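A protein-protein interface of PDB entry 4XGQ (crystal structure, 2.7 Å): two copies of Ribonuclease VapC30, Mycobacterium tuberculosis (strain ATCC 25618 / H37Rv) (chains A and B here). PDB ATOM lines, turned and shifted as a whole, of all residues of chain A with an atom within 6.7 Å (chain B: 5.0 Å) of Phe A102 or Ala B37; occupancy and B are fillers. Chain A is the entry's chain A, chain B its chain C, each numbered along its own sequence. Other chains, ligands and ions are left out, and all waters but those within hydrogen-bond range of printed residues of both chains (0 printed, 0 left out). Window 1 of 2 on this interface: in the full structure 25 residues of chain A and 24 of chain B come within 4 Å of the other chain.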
ATOM      1  N   VAL A   3       2.476  22.178 -32.314  1.00  0.00           N
ATOM      2  CA  VAL A   3       1.622  21.437 -31.430  1.00  0.00           C
ATOM      3  C   VAL A   3       1.647  20.001 -31.917  1.00  0.00           C
ATOM      4  O   VAL A   3       1.526  19.766 -33.100  1.00  0.00           O
ATOM      5  CB  VAL A   3       0.173  22.015 -31.447  1.00  0.00           C
ATOM      6  CG1 VAL A   3      -0.809  21.189 -30.605  1.00  0.00           C
ATOM      7  CG2 VAL A   3       0.219  23.438 -30.950  1.00  0.00           C
ATOM      8  N   ASP A   5      -0.032  16.136 -31.970  1.00  0.00           N
ATOM      9  CA  ASP A   5      -1.297  15.476 -31.769  1.00  0.00           C
ATOM     10  C   ASP A   5      -1.087  14.043 -31.399  1.00  0.00           C
ATOM     11  O   ASP A   5      -0.016  13.485 -31.609  1.00  0.00           O
ATOM     12  CB  ASP A   5      -2.147  15.526 -33.028  1.00  0.00           C
ATOM     13  CG  ASP A   5      -3.571  15.036 -32.791  1.00  0.00           C
ATOM     14  OD1 ASP A   5      -4.209  15.535 -31.832  1.00  0.00           O
ATOM     15  OD2 ASP A   5      -4.050  14.167 -33.552  1.00  0.00           O
ATOM     16  N   SER A  35      -1.468  19.210 -25.762  1.00  0.00           N
ATOM     17  CA  SER A  35      -2.551  19.386 -24.806  1.00  0.00           C
ATOM     18  C   SER A  35      -2.616  18.221 -23.903  1.00  0.00           C
ATOM     19  O   SER A  35      -2.467  17.090 -24.350  1.00  0.00           O
ATOM     20  CB  SER A  35      -3.899  19.499 -25.489  1.00  0.00           C
ATOM     21  OG  SER A  35      -4.902  19.669 -24.514  1.00  0.00           O
ATOM     22  N   THR A  36      -2.891  18.504 -22.631  1.00  0.00           N
ATOM     23  CA  THR A  36      -2.955  17.481 -21.567  1.00  0.00           C
ATOM     24  C   THR A  36      -3.938  16.381 -21.920  1.00  0.00           C
ATOM     25  O   THR A  36      -3.767  15.250 -21.520  1.00  0.00           O
ATOM     26  CB  THR A  36      -3.345  18.109 -20.204  1.00  0.00           C
ATOM     27  OG1 THR A  36      -4.465  19.000 -20.361  1.00  0.00           O
ATOM     28  CG2 THR A  36      -2.217  18.910 -19.633  1.00  0.00           C
ATOM     29  N   ALA A  37      -4.981  16.732 -22.655  1.00  0.00           N
ATOM     30  CA  ALA A  37      -5.977  15.755 -23.073  1.00  0.00           C
ATOM     31  C   ALA A  37      -5.485  14.850 -24.211  1.00  0.00           C
ATOM     32  O   ALA A  37      -5.962  13.726 -24.360  1.00  0.00           O
ATOM     33  CB  ALA A  37      -7.260  16.472 -23.484  1.00  0.00           C
ATOM     34  N   SER A  38      -4.585  15.362 -25.051  1.00  0.00           N
ATOM     35  CA  SER A  38      -4.013  14.574 -26.154  1.00  0.00           C
ATOM     36  C   SER A  38      -2.987  13.635 -25.601  1.00  0.00           C
ATOM     37  O   SER A  38      -2.945  12.481 -26.008  1.00  0.00           O
ATOM     38  CB  SER A  38      -3.423  15.467 -27.217  1.00  0.00           C
ATOM     39  OG  SER A  38      -4.478  16.008 -28.019  1.00  0.00           O
ATOM     40  N   GLU A  41      -5.051  10.820 -24.082  1.00  0.00           N
ATOM     41  CA  GLU A  41      -5.541   9.915 -25.128  1.00  0.00           C
ATOM     42  C   GLU A  41      -4.422   9.036 -25.632  1.00  0.00           C
ATOM     43  O   GLU A  41      -4.652   7.885 -25.914  1.00  0.00           O
ATOM     44  CB  GLU A  41      -6.139  10.692 -26.313  1.00  0.00           C
ATOM     45  CG  GLU A  41      -7.042   9.827 -27.196  1.00  0.00           C
ATOM     46  CD  GLU A  41      -7.418  10.452 -28.549  1.00  0.00           C
ATOM     47  OE1 GLU A  41      -7.309  11.706 -28.738  1.00  0.00           O
ATOM     48  OE2 GLU A  41      -7.829   9.668 -29.451  1.00  0.00           O
ATOM     49  N   VAL A  72      -5.851  22.494 -20.684  1.00  0.00           N
ATOM     50  CA  VAL A  72      -6.994  22.867 -21.512  1.00  0.00           C
ATOM     51  C   VAL A  72      -7.835  23.919 -20.755  1.00  0.00           C
ATOM     52  O   VAL A  72      -8.484  23.625 -19.742  1.00  0.00           O
ATOM     53  CB  VAL A  72      -7.888  21.659 -21.817  1.00  0.00           C
ATOM     54  CG1 VAL A  72      -8.935  22.032 -22.859  1.00  0.00           C
ATOM     55  CG2 VAL A  72      -7.066  20.498 -22.332  1.00  0.00           C
ATOM     56  N   GLN A  76      -9.703  27.534 -25.043  1.00  0.00           N
ATOM     57  CA  GLN A  76      -9.412  26.442 -25.974  1.00  0.00           C
ATOM     58  C   GLN A  76     -10.654  25.622 -26.198  1.00  0.00           C
ATOM     59  O   GLN A  76     -10.924  25.225 -27.327  1.00  0.00           O
ATOM     60  CB  GLN A  76      -8.310  25.498 -25.447  1.00  0.00           C
ATOM     61  CG  GLN A  76      -6.900  26.061 -25.292  1.00  0.00           C
ATOM     62  CD  GLN A  76      -5.990  25.097 -24.552  1.00  0.00           C
ATOM     63  OE1 GLN A  76      -5.969  23.888 -24.854  1.00  0.00           O
ATOM     64  NE2 GLN A  76      -5.241  25.610 -23.571  1.00  0.00           N
ATOM     65  N   ALA A  77     -11.404  25.349 -25.139  1.00  0.00           N
ATOM     66  CA  ALA A  77     -12.638  24.602 -25.308  1.00  0.00           C
ATOM     67  C   ALA A  77     -13.673  25.376 -26.137  1.00  0.00           C
ATOM     68  O   ALA A  77     -14.363  24.762 -26.971  1.00  0.00           O
ATOM     69  CB  ALA A  77     -13.196  24.224 -23.962  1.00  0.00           C
ATOM     70  N   ALA A  80     -12.648  25.119 -29.888  1.00  0.00           N
ATOM     71  CA  ALA A  80     -12.945  23.740 -30.238  1.00  0.00           C
ATOM     72  C   ALA A  80     -14.448  23.496 -30.516  1.00  0.00           C
ATOM     73  O   ALA A  80     -14.819  22.839 -31.507  1.00  0.00           O
ATOM     74  CB  ALA A  80     -12.469  22.833 -29.127  1.00  0.00           C
ATOM     75  N   ASN A  97     -12.892  14.701 -34.400  1.00  0.00           N
ATOM     76  CA  ASN A  97     -13.747  14.077 -33.387  1.00  0.00           C
ATOM     77  C   ASN A  97     -13.499  14.672 -31.986  1.00  0.00           C
ATOM     78  O   ASN A  97     -12.759  15.660 -31.823  1.00  0.00           O
ATOM     79  CB  ASN A  97     -13.604  12.572 -33.421  1.00  0.00           C
ATOM     80  CG  ASN A  97     -12.209  12.109 -33.098  1.00  0.00           C
ATOM     81  OD1 ASN A  97     -11.461  12.762 -32.361  1.00  0.00           O
ATOM     82  ND2 ASN A  97     -11.853  10.966 -33.641  1.00  0.00           N
ATOM     83  N   TYR A  98     -14.155  14.127 -30.974  1.00  0.00           N
ATOM     84  CA  TYR A  98     -14.025  14.670 -29.615  1.00  0.00           C
ATOM     85  C   TYR A  98     -12.559  14.885 -29.195  1.00  0.00           C
ATOM     86  O   TYR A  98     -12.203  15.946 -28.669  1.00  0.00           O
ATOM     87  CB  TYR A  98     -14.744  13.761 -28.603  1.00  0.00           C
ATOM     88  CG  TYR A  98     -14.643  14.242 -27.154  1.00  0.00           C
ATOM     89  CD1 TYR A  98     -14.919  15.552 -26.819  1.00  0.00           C
ATOM     90  CD2 TYR A  98     -14.262  13.390 -26.138  1.00  0.00           C
ATOM     91  CE1 TYR A  98     -14.821  15.998 -25.518  1.00  0.00           C
ATOM     92  CE2 TYR A  98     -14.182  13.831 -24.828  1.00  0.00           C
ATOM     93  CZ  TYR A  98     -14.465  15.140 -24.535  1.00  0.00           C
ATOM     94  OH  TYR A  98     -14.390  15.632 -23.263  1.00  0.00           O
ATOM     95  N   GLY A  99     -11.718  13.882 -29.429  1.00  0.00           N
ATOM     96  CA  GLY A  99     -10.311  13.957 -29.047  1.00  0.00           C
ATOM     97  C   GLY A  99      -9.537  15.008 -29.811  1.00  0.00           C
ATOM     98  O   GLY A  99      -8.781  15.789 -29.238  1.00  0.00           O
ATOM     99  N   ASP A 100      -9.748  15.056 -31.116  1.00  0.00           N
ATOM    100  CA  ASP A 100      -9.039  16.005 -31.954  1.00  0.00           C
ATOM    101  C   ASP A 100      -9.232  17.409 -31.435  1.00  0.00           C
ATOM    102  O   ASP A 100      -8.328  18.244 -31.480  1.00  0.00           O
ATOM    103  CB  ASP A 100      -9.556  15.888 -33.382  1.00  0.00           C
ATOM    104  CG  ASP A 100      -9.314  14.502 -33.976  1.00  0.00           C
ATOM    105  OD1 ASP A 100      -8.277  13.908 -33.619  1.00  0.00           O
ATOM    106  OD2 ASP A 100     -10.149  14.010 -34.788  1.00  0.00           O
ATOM    107  N   CYS A 101     -10.432  17.678 -30.936  1.00  0.00           N
ATOM    108  CA  CYS A 101     -10.791  19.035 -30.474  1.00  0.00           C
ATOM    109  C   CYS A 101      -9.755  19.614 -29.526  1.00  0.00           C
ATOM    110  O   CYS A 101      -9.553  20.836 -29.485  1.00  0.00           O
ATOM    111  CB  CYS A 101     -12.166  19.064 -29.793  1.00  0.00           C
ATOM    112  SG  CYS A 101     -13.530  18.806 -30.940  1.00  0.00           S
ATOM    113  N   PHE A 102      -9.106  18.749 -28.755  1.00  0.00           N
ATOM    114  CA  PHE A 102      -8.219  19.230 -27.727  1.00  0.00           C
ATOM    115  C   PHE A 102      -6.924  19.793 -28.288  1.00  0.00           C
ATOM    116  O   PHE A 102      -6.460  20.848 -27.806  1.00  0.00           O
ATOM    117  CB  PHE A 102      -7.997  18.148 -26.680  1.00  0.00           C
ATOM    118  CG  PHE A 102      -9.233  17.825 -25.921  1.00  0.00           C
ATOM    119  CD1 PHE A 102      -9.792  18.753 -25.051  1.00  0.00           C
ATOM    120  CD2 PHE A 102      -9.868  16.640 -26.107  1.00  0.00           C
ATOM    121  CE1 PHE A 102     -10.957  18.466 -24.376  1.00  0.00           C
ATOM    122  CE2 PHE A 102     -11.030  16.343 -25.422  1.00  0.00           C
ATOM    123  CZ  PHE A 102     -11.578  17.257 -24.563  1.00  0.00           C
ATOM    124  N   SER A 103      -6.386  19.132 -29.322  1.00  0.00           N
ATOM    125  CA  SER A 103      -5.217  19.670 -30.051  1.00  0.00           C
ATOM    126  C   SER A 103      -5.594  20.849 -30.966  1.00  0.00           C
ATOM    127  O   SER A 103      -4.826  21.814 -31.117  1.00  0.00           O
ATOM    128  CB  SER A 103      -4.485  18.575 -30.816  1.00  0.00           C
ATOM    129  OG  SER A 103      -3.638  17.858 -29.903  1.00  0.00           O
ATOM    130  N   TYR A 104      -6.779  20.790 -31.557  1.00  0.00           N
ATOM    131  CA  TYR A 104      -7.260  21.894 -32.379  1.00  0.00           C
ATOM    132  C   TYR A 104      -7.374  23.157 -31.551  1.00  0.00           C
ATOM    133  O   TYR A 104      -6.983  24.251 -31.995  1.00  0.00           O
ATOM    134  CB  TYR A 104      -8.631  21.583 -32.989  1.00  0.00           C
ATOM    135  CG  TYR A 104      -9.199  22.790 -33.710  1.00  0.00           C
ATOM    136  CD1 TYR A 104      -9.862  23.804 -33.001  1.00  0.00           C
ATOM    137  CD2 TYR A 104      -9.051  22.947 -35.106  1.00  0.00           C
ATOM    138  CE1 TYR A 104     -10.351  24.934 -33.643  1.00  0.00           C
ATOM    139  CE2 TYR A 104      -9.552  24.070 -35.754  1.00  0.00           C
ATOM    140  CZ  TYR A 104     -10.197  25.057 -35.014  1.00  0.00           C
ATOM    141  OH  TYR A 104     -10.663  26.168 -35.641  1.00  0.00           O
ATOM    142  N   GLY A 105      -7.951  23.017 -30.356  1.00  0.00           N
ATOM    143  CA  GLY A 105      -8.176  24.155 -29.469  1.00  0.00           C
ATOM    144  C   GLY A 105      -6.854  24.768 -29.087  1.00  0.00           C
ATOM    145  O   GLY A 105      -6.685  25.972 -29.193  1.00  0.00           O
ATOM    146  N   LEU A 106      -5.901  23.938 -28.668  1.00  0.00           N
ATOM    147  CA  LEU A 106      -4.565  24.409 -28.309  1.00  0.00           C
ATOM    148  C   LEU A 106      -3.903  25.080 -29.512  1.00  0.00           C
ATOM    149  O   LEU A 106      -3.334  26.165 -29.375  1.00  0.00           O
ATOM    150  CB  LEU A 106      -3.707  23.254 -27.826  1.00  0.00           C
ATOM    151  CG  LEU A 106      -2.287  23.578 -27.365  1.00  0.00           C
ATOM    152  CD1 LEU A 106      -2.285  24.607 -26.236  1.00  0.00           C
ATOM    153  CD2 LEU A 106      -1.613  22.289 -26.912  1.00  0.00           C
ATOM    154  N   ALA A 107      -3.979  24.429 -30.680  1.00  0.00           N
ATOM    155  CA  ALA A 107      -3.404  24.979 -31.915  1.00  0.00           C
ATOM    156  C   ALA A 107      -4.066  26.302 -32.300  1.00  0.00           C
ATOM    157  O   ALA A 107      -3.390  27.228 -32.738  1.00  0.00           O
ATOM    158  CB  ALA A 107      -3.554  23.968 -33.055  1.00  0.00           C
ATOM    159  N   PHE A 121      -7.458  16.535 -39.576  1.00  0.00           N
ATOM    160  CA  PHE A 121      -7.139  17.967 -39.463  1.00  0.00           C
ATOM    161  C   PHE A 121      -6.827  18.665 -40.778  1.00  0.00           C
ATOM    162  O   PHE A 121      -6.489  19.867 -40.765  1.00  0.00           O
ATOM    163  CB  PHE A 121      -5.927  18.151 -38.552  1.00  0.00           C
ATOM    164  CG  PHE A 121      -6.123  17.644 -37.161  1.00  0.00           C
ATOM    165  CD1 PHE A 121      -5.887  16.310 -36.853  1.00  0.00           C
ATOM    166  CD2 PHE A 121      -6.525  18.508 -36.160  1.00  0.00           C
ATOM    167  CE1 PHE A 121      -6.037  15.858 -35.557  1.00  0.00           C
ATOM    168  CE2 PHE A 121      -6.677  18.056 -34.856  1.00  0.00           C
ATOM    169  CZ  PHE A 121      -6.436  16.733 -34.559  1.00  0.00           C
ATOM    170  N   SER B  35     -15.218  20.288 -15.505  1.00  0.00           N
ATOM    171  CA  SER B  35     -13.948  20.281 -16.228  1.00  0.00           C
ATOM    172  C   SER B  35     -14.141  20.914 -17.558  1.00  0.00           C
ATOM    173  O   SER B  35     -15.053  20.534 -18.299  1.00  0.00           O
ATOM    174  CB  SER B  35     -13.456  18.837 -16.461  1.00  0.00           C
ATOM    175  OG  SER B  35     -12.345  18.786 -17.344  1.00  0.00           O
ATOM    176  N   THR B  36     -13.246  21.809 -17.926  1.00  0.00           N
ATOM    177  CA  THR B  36     -13.344  22.425 -19.261  1.00  0.00           C
ATOM    178  C   THR B  36     -13.599  21.435 -20.375  1.00  0.00           C
ATOM    179  O   THR B  36     -14.186  21.803 -21.384  1.00  0.00           O
ATOM    180  CB  THR B  36     -12.091  23.196 -19.610  1.00  0.00           C
ATOM    181  OG1 THR B  36     -10.965  22.390 -19.264  1.00  0.00           O
ATOM    182  CG2 THR B  36     -12.040  24.490 -18.844  1.00  0.00           C
ATOM    183  N   ALA B  37     -13.131  20.205 -20.208  1.00  0.00           N
ATOM    184  CA  ALA B  37     -13.319  19.177 -21.228  1.00  0.00           C
ATOM    185  C   ALA B  37     -14.716  18.570 -21.155  1.00  0.00           C
ATOM    186  O   ALA B  37     -15.254  18.132 -22.164  1.00  0.00           O
ATOM    187  CB  ALA B  37     -12.266  18.068 -21.090  1.00  0.00           C
ATOM    188  N   SER B  38     -15.267  18.474 -19.948  1.00  0.00           N
ATOM    189  CA  SER B  38     -16.650  18.014 -19.766  1.00  0.00           C
ATOM    190  C   SER B  38     -17.616  19.047 -20.393  1.00  0.00           C
ATOM    191  O   SER B  38     -18.526  18.703 -21.129  1.00  0.00           O
ATOM    192  CB  SER B  38     -16.950  17.835 -18.273  1.00  0.00           C
ATOM    193  OG  SER B  38     -16.232  16.749 -17.687  1.00  0.00           O
ATOM    194  N   TYR B  39     -17.374  20.325 -20.127  1.00  0.00           N
ATOM    195  CA  TYR B  39     -18.051  21.405 -20.849  1.00  0.00           C
ATOM    196  C   TYR B  39     -18.088  21.151 -22.347  1.00  0.00           C
ATOM    197  O   TYR B  39     -19.148  21.133 -22.952  1.00  0.00           O
ATOM    198  CB  TYR B  39     -17.401  22.751 -20.530  1.00  0.00           C
ATOM    199  CG  TYR B  39     -17.573  23.800 -21.584  1.00  0.00           C
ATOM    200  CD1 TYR B  39     -18.819  24.356 -21.851  1.00  0.00           C
ATOM    201  CD2 TYR B  39     -16.490  24.281 -22.292  1.00  0.00           C
ATOM    202  CE1 TYR B  39     -18.974  25.349 -22.826  1.00  0.00           C
ATOM    203  CE2 TYR B  39     -16.636  25.276 -23.259  1.00  0.00           C
ATOM    204  CZ  TYR B  39     -17.877  25.809 -23.532  1.00  0.00           C
ATOM    205  OH  TYR B  39     -18.010  26.773 -24.516  1.00  0.00           O
ATOM    206  N   LEU B  40     -16.934  20.906 -22.940  1.00  0.00           N
ATOM    207  CA  LEU B  40     -16.852  20.686 -24.376  1.00  0.00           C
ATOM    208  C   LEU B  40     -17.726  19.548 -24.805  1.00  0.00           C
ATOM    209  O   LEU B  40     -18.552  19.690 -25.674  1.00  0.00           O
ATOM    210  CB  LEU B  40     -15.401  20.387 -24.786  1.00  0.00           C
ATOM    211  CG  LEU B  40     -15.116  19.990 -26.243  1.00  0.00           C
ATOM    212  CD1 LEU B  40     -15.435  21.158 -27.161  1.00  0.00           C
ATOM    213  CD2 LEU B  40     -13.659  19.606 -26.406  1.00  0.00           C
ATOM    214  N   GLU B  41     -17.515  18.396 -24.208  1.00  0.00           N
ATOM    215  CA  GLU B  41     -18.272  17.189 -24.576  1.00  0.00           C
ATOM    216  C   GLU B  41     -19.774  17.472 -24.583  1.00  0.00           C
ATOM    217  O   GLU B  41     -20.501  17.086 -25.518  1.00  0.00           O
ATOM    218  CB  GLU B  41     -17.979  16.029 -23.596  1.00  0.00           C
ATOM    219  CG  GLU B  41     -18.296  14.637 -24.175  1.00  0.00           C
ATOM    220  CD  GLU B  41     -18.307  13.536 -23.123  1.00  0.00           C
ATOM    221  OE1 GLU B  41     -17.818  13.729 -21.976  1.00  0.00           O
ATOM    222  OE2 GLU B  41     -18.836  12.474 -23.449  1.00  0.00           O
ATOM    223  N   VAL B  72      -8.093  21.453 -17.396  1.00  0.00           N
ATOM    224  CA  VAL B  72      -7.546  20.119 -17.261  1.00  0.00           C
ATOM    225  C   VAL B  72      -6.029  20.275 -17.139  1.00  0.00           C
ATOM    226  O   VAL B  72      -5.321  20.440 -18.137  1.00  0.00           O
ATOM    227  CB  VAL B  72      -7.865  19.261 -18.479  1.00  0.00           C
ATOM    228  CG1 VAL B  72      -7.375  17.855 -18.255  1.00  0.00           C
ATOM    229  CG2 VAL B  72      -9.346  19.242 -18.767  1.00  0.00           C
ATOM    230  N   TYR B  98     -13.185   7.815 -22.323  1.00  0.00           N
ATOM    231  CA  TYR B  98     -12.279   8.956 -22.448  1.00  0.00           C
ATOM    232  C   TYR B  98     -12.899  10.239 -21.899  1.00  0.00           C
ATOM    233  O   TYR B  98     -12.243  11.001 -21.190  1.00  0.00           O
ATOM    234  CB  TYR B  98     -11.893   9.135 -23.927  1.00  0.00           C
ATOM    235  CG  TYR B  98     -10.977  10.305 -24.224  1.00  0.00           C
ATOM    236  CD1 TYR B  98      -9.789  10.456 -23.555  1.00  0.00           C
ATOM    237  CD2 TYR B  98     -11.297  11.237 -25.181  1.00  0.00           C
ATOM    238  CE1 TYR B  98      -8.945  11.518 -23.808  1.00  0.00           C
ATOM    239  CE2 TYR B  98     -10.447  12.289 -25.451  1.00  0.00           C
ATOM    240  CZ  TYR B  98      -9.272  12.423 -24.754  1.00  0.00           C
ATOM    241  OH  TYR B  98      -8.398  13.455 -25.006  1.00  0.00           O
ATOM    242  N   PHE B 102     -11.960  12.795 -17.718  1.00  0.00           N
ATOM    243  CA  PHE B 102     -11.757  14.170 -17.285  1.00  0.00           C
ATOM    244  C   PHE B 102     -12.606  14.570 -16.054  1.00  0.00           C
ATOM    245  O   PHE B 102     -12.126  15.341 -15.201  1.00  0.00           O
ATOM    246  CB  PHE B 102     -12.031  15.086 -18.430  1.00  0.00           C
ATOM    247  CG  PHE B 102     -11.159  14.827 -19.606  1.00  0.00           C
ATOM    248  CD1 PHE B 102      -9.905  15.402 -19.673  1.00  0.00           C
ATOM    249  CD2 PHE B 102     -11.599  14.020 -20.663  1.00  0.00           C
ATOM    250  CE1 PHE B 102      -9.099  15.173 -20.771  1.00  0.00           C
ATOM    251  CE2 PHE B 102     -10.803  13.804 -21.771  1.00  0.00           C
ATOM    252  CZ  PHE B 102      -9.551  14.376 -21.824  1.00  0.00           C
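Of the printed residues of chain B, Ala A77 touches Thr B36, Tyr B39 and Leu B40.
Of chain A, only Tyr A98 and Phe A102 come within 4 Å of Ala B37.
Of the printed residues of chain A, Phe B102 touches Ala A37.
The nearest printed residue of chain A that does not touch Val B72 is Ala A37 (5.1 Å).
Among the printed residues, pairs that only touch across the chains: Ala A37 with Phe B102 (3.5 Å), Glu A41 with Tyr B98 (3.8 Å), Ala A77 with Thr B36 (3.7 Å), Ala A77 with Tyr B39 (3.7 Å), Ala A77 with Leu B40 (3.8 Å), Ala A80 with Leu B40 (3.9 Å), Tyr A98 with Leu B40 (3.9 Å), Tyr A98 with Glu B41 (3.6 Å), Tyr A98 with Tyr B98 (3.8 Å), Gly A99 with Tyr B98 (3.97 Å), Cys A101 with Leu B40 (3.7 Å), Phe A102 with Ala B37 (3.6 Å), Phe A102 with Leu B40 (3.6 Å) and Phe A102 with Tyr B98 (3.7 Å).
The side-chain hydroxyl (OG) of Ser A35 sits close to the backbone NH (N) of Ala A37, 3.5 Å away.
The side-chain amide oxygen (OD1) of Asn A97 is in hydrogen-bond range of the backbone NH (N) of Gly A99, 3.1 Å away.
The backbone carbonyl oxygen (O) of Asn A97 sits at hydrogen-bond distance from the side-chain sulfur (SG) of Cys A101, 3.4 Å away.
The side-chain hydroxyl of Ser B35 lies close to the backbone NH of Ala B37, 3.3 Å away.
Of the 10 printed residues of chain B, 8 touch a printed residue of chain A.
Hydrophobic or aromatic side chains of chain B within 4 Å of the printed part of chain A: Ala B37, Tyr B39, Leu B40, Val B72, Tyr B98 and Phe B102.
Of the 23 printed residues of chain A, 10 touch a printed residue of chain B.
Thr A36 touches Val B72, and with the chains exchanged Val A72 touches Thr B36.
Ala A37 touches Tyr B98, and with the chains exchanged Tyr A98 touches Ala B37.
Val B72 touches its own counterpart, Val A72.
Phe A102 touches Tyr B98, but with the chains exchanged Tyr A98 does not touch Phe B102 (4.1 Å).
8 positions are printed for both chains.
Of the 19 pairs that touch across the chains among the printed residues, 10 have their exchanged pair printed and touching as well.
O of Val B72 is in hydrogen-bond range of OG1 of Thr A36, at 2.8 Å.
O of Ala A37 sits at hydrogen-bond distance from OH of Tyr B98 (2.5 Å).
OG1 of Thr B36 lies within hydrogen-bond range of O of Val A72, at 2.8 Å.
The backbone NH (N) of Val B72 lies within hydrogen-bond range of the backbone carbonyl oxygen (O) of Val A72.
O of Ala B37 sits at hydrogen-bond distance from OH of Tyr A98.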
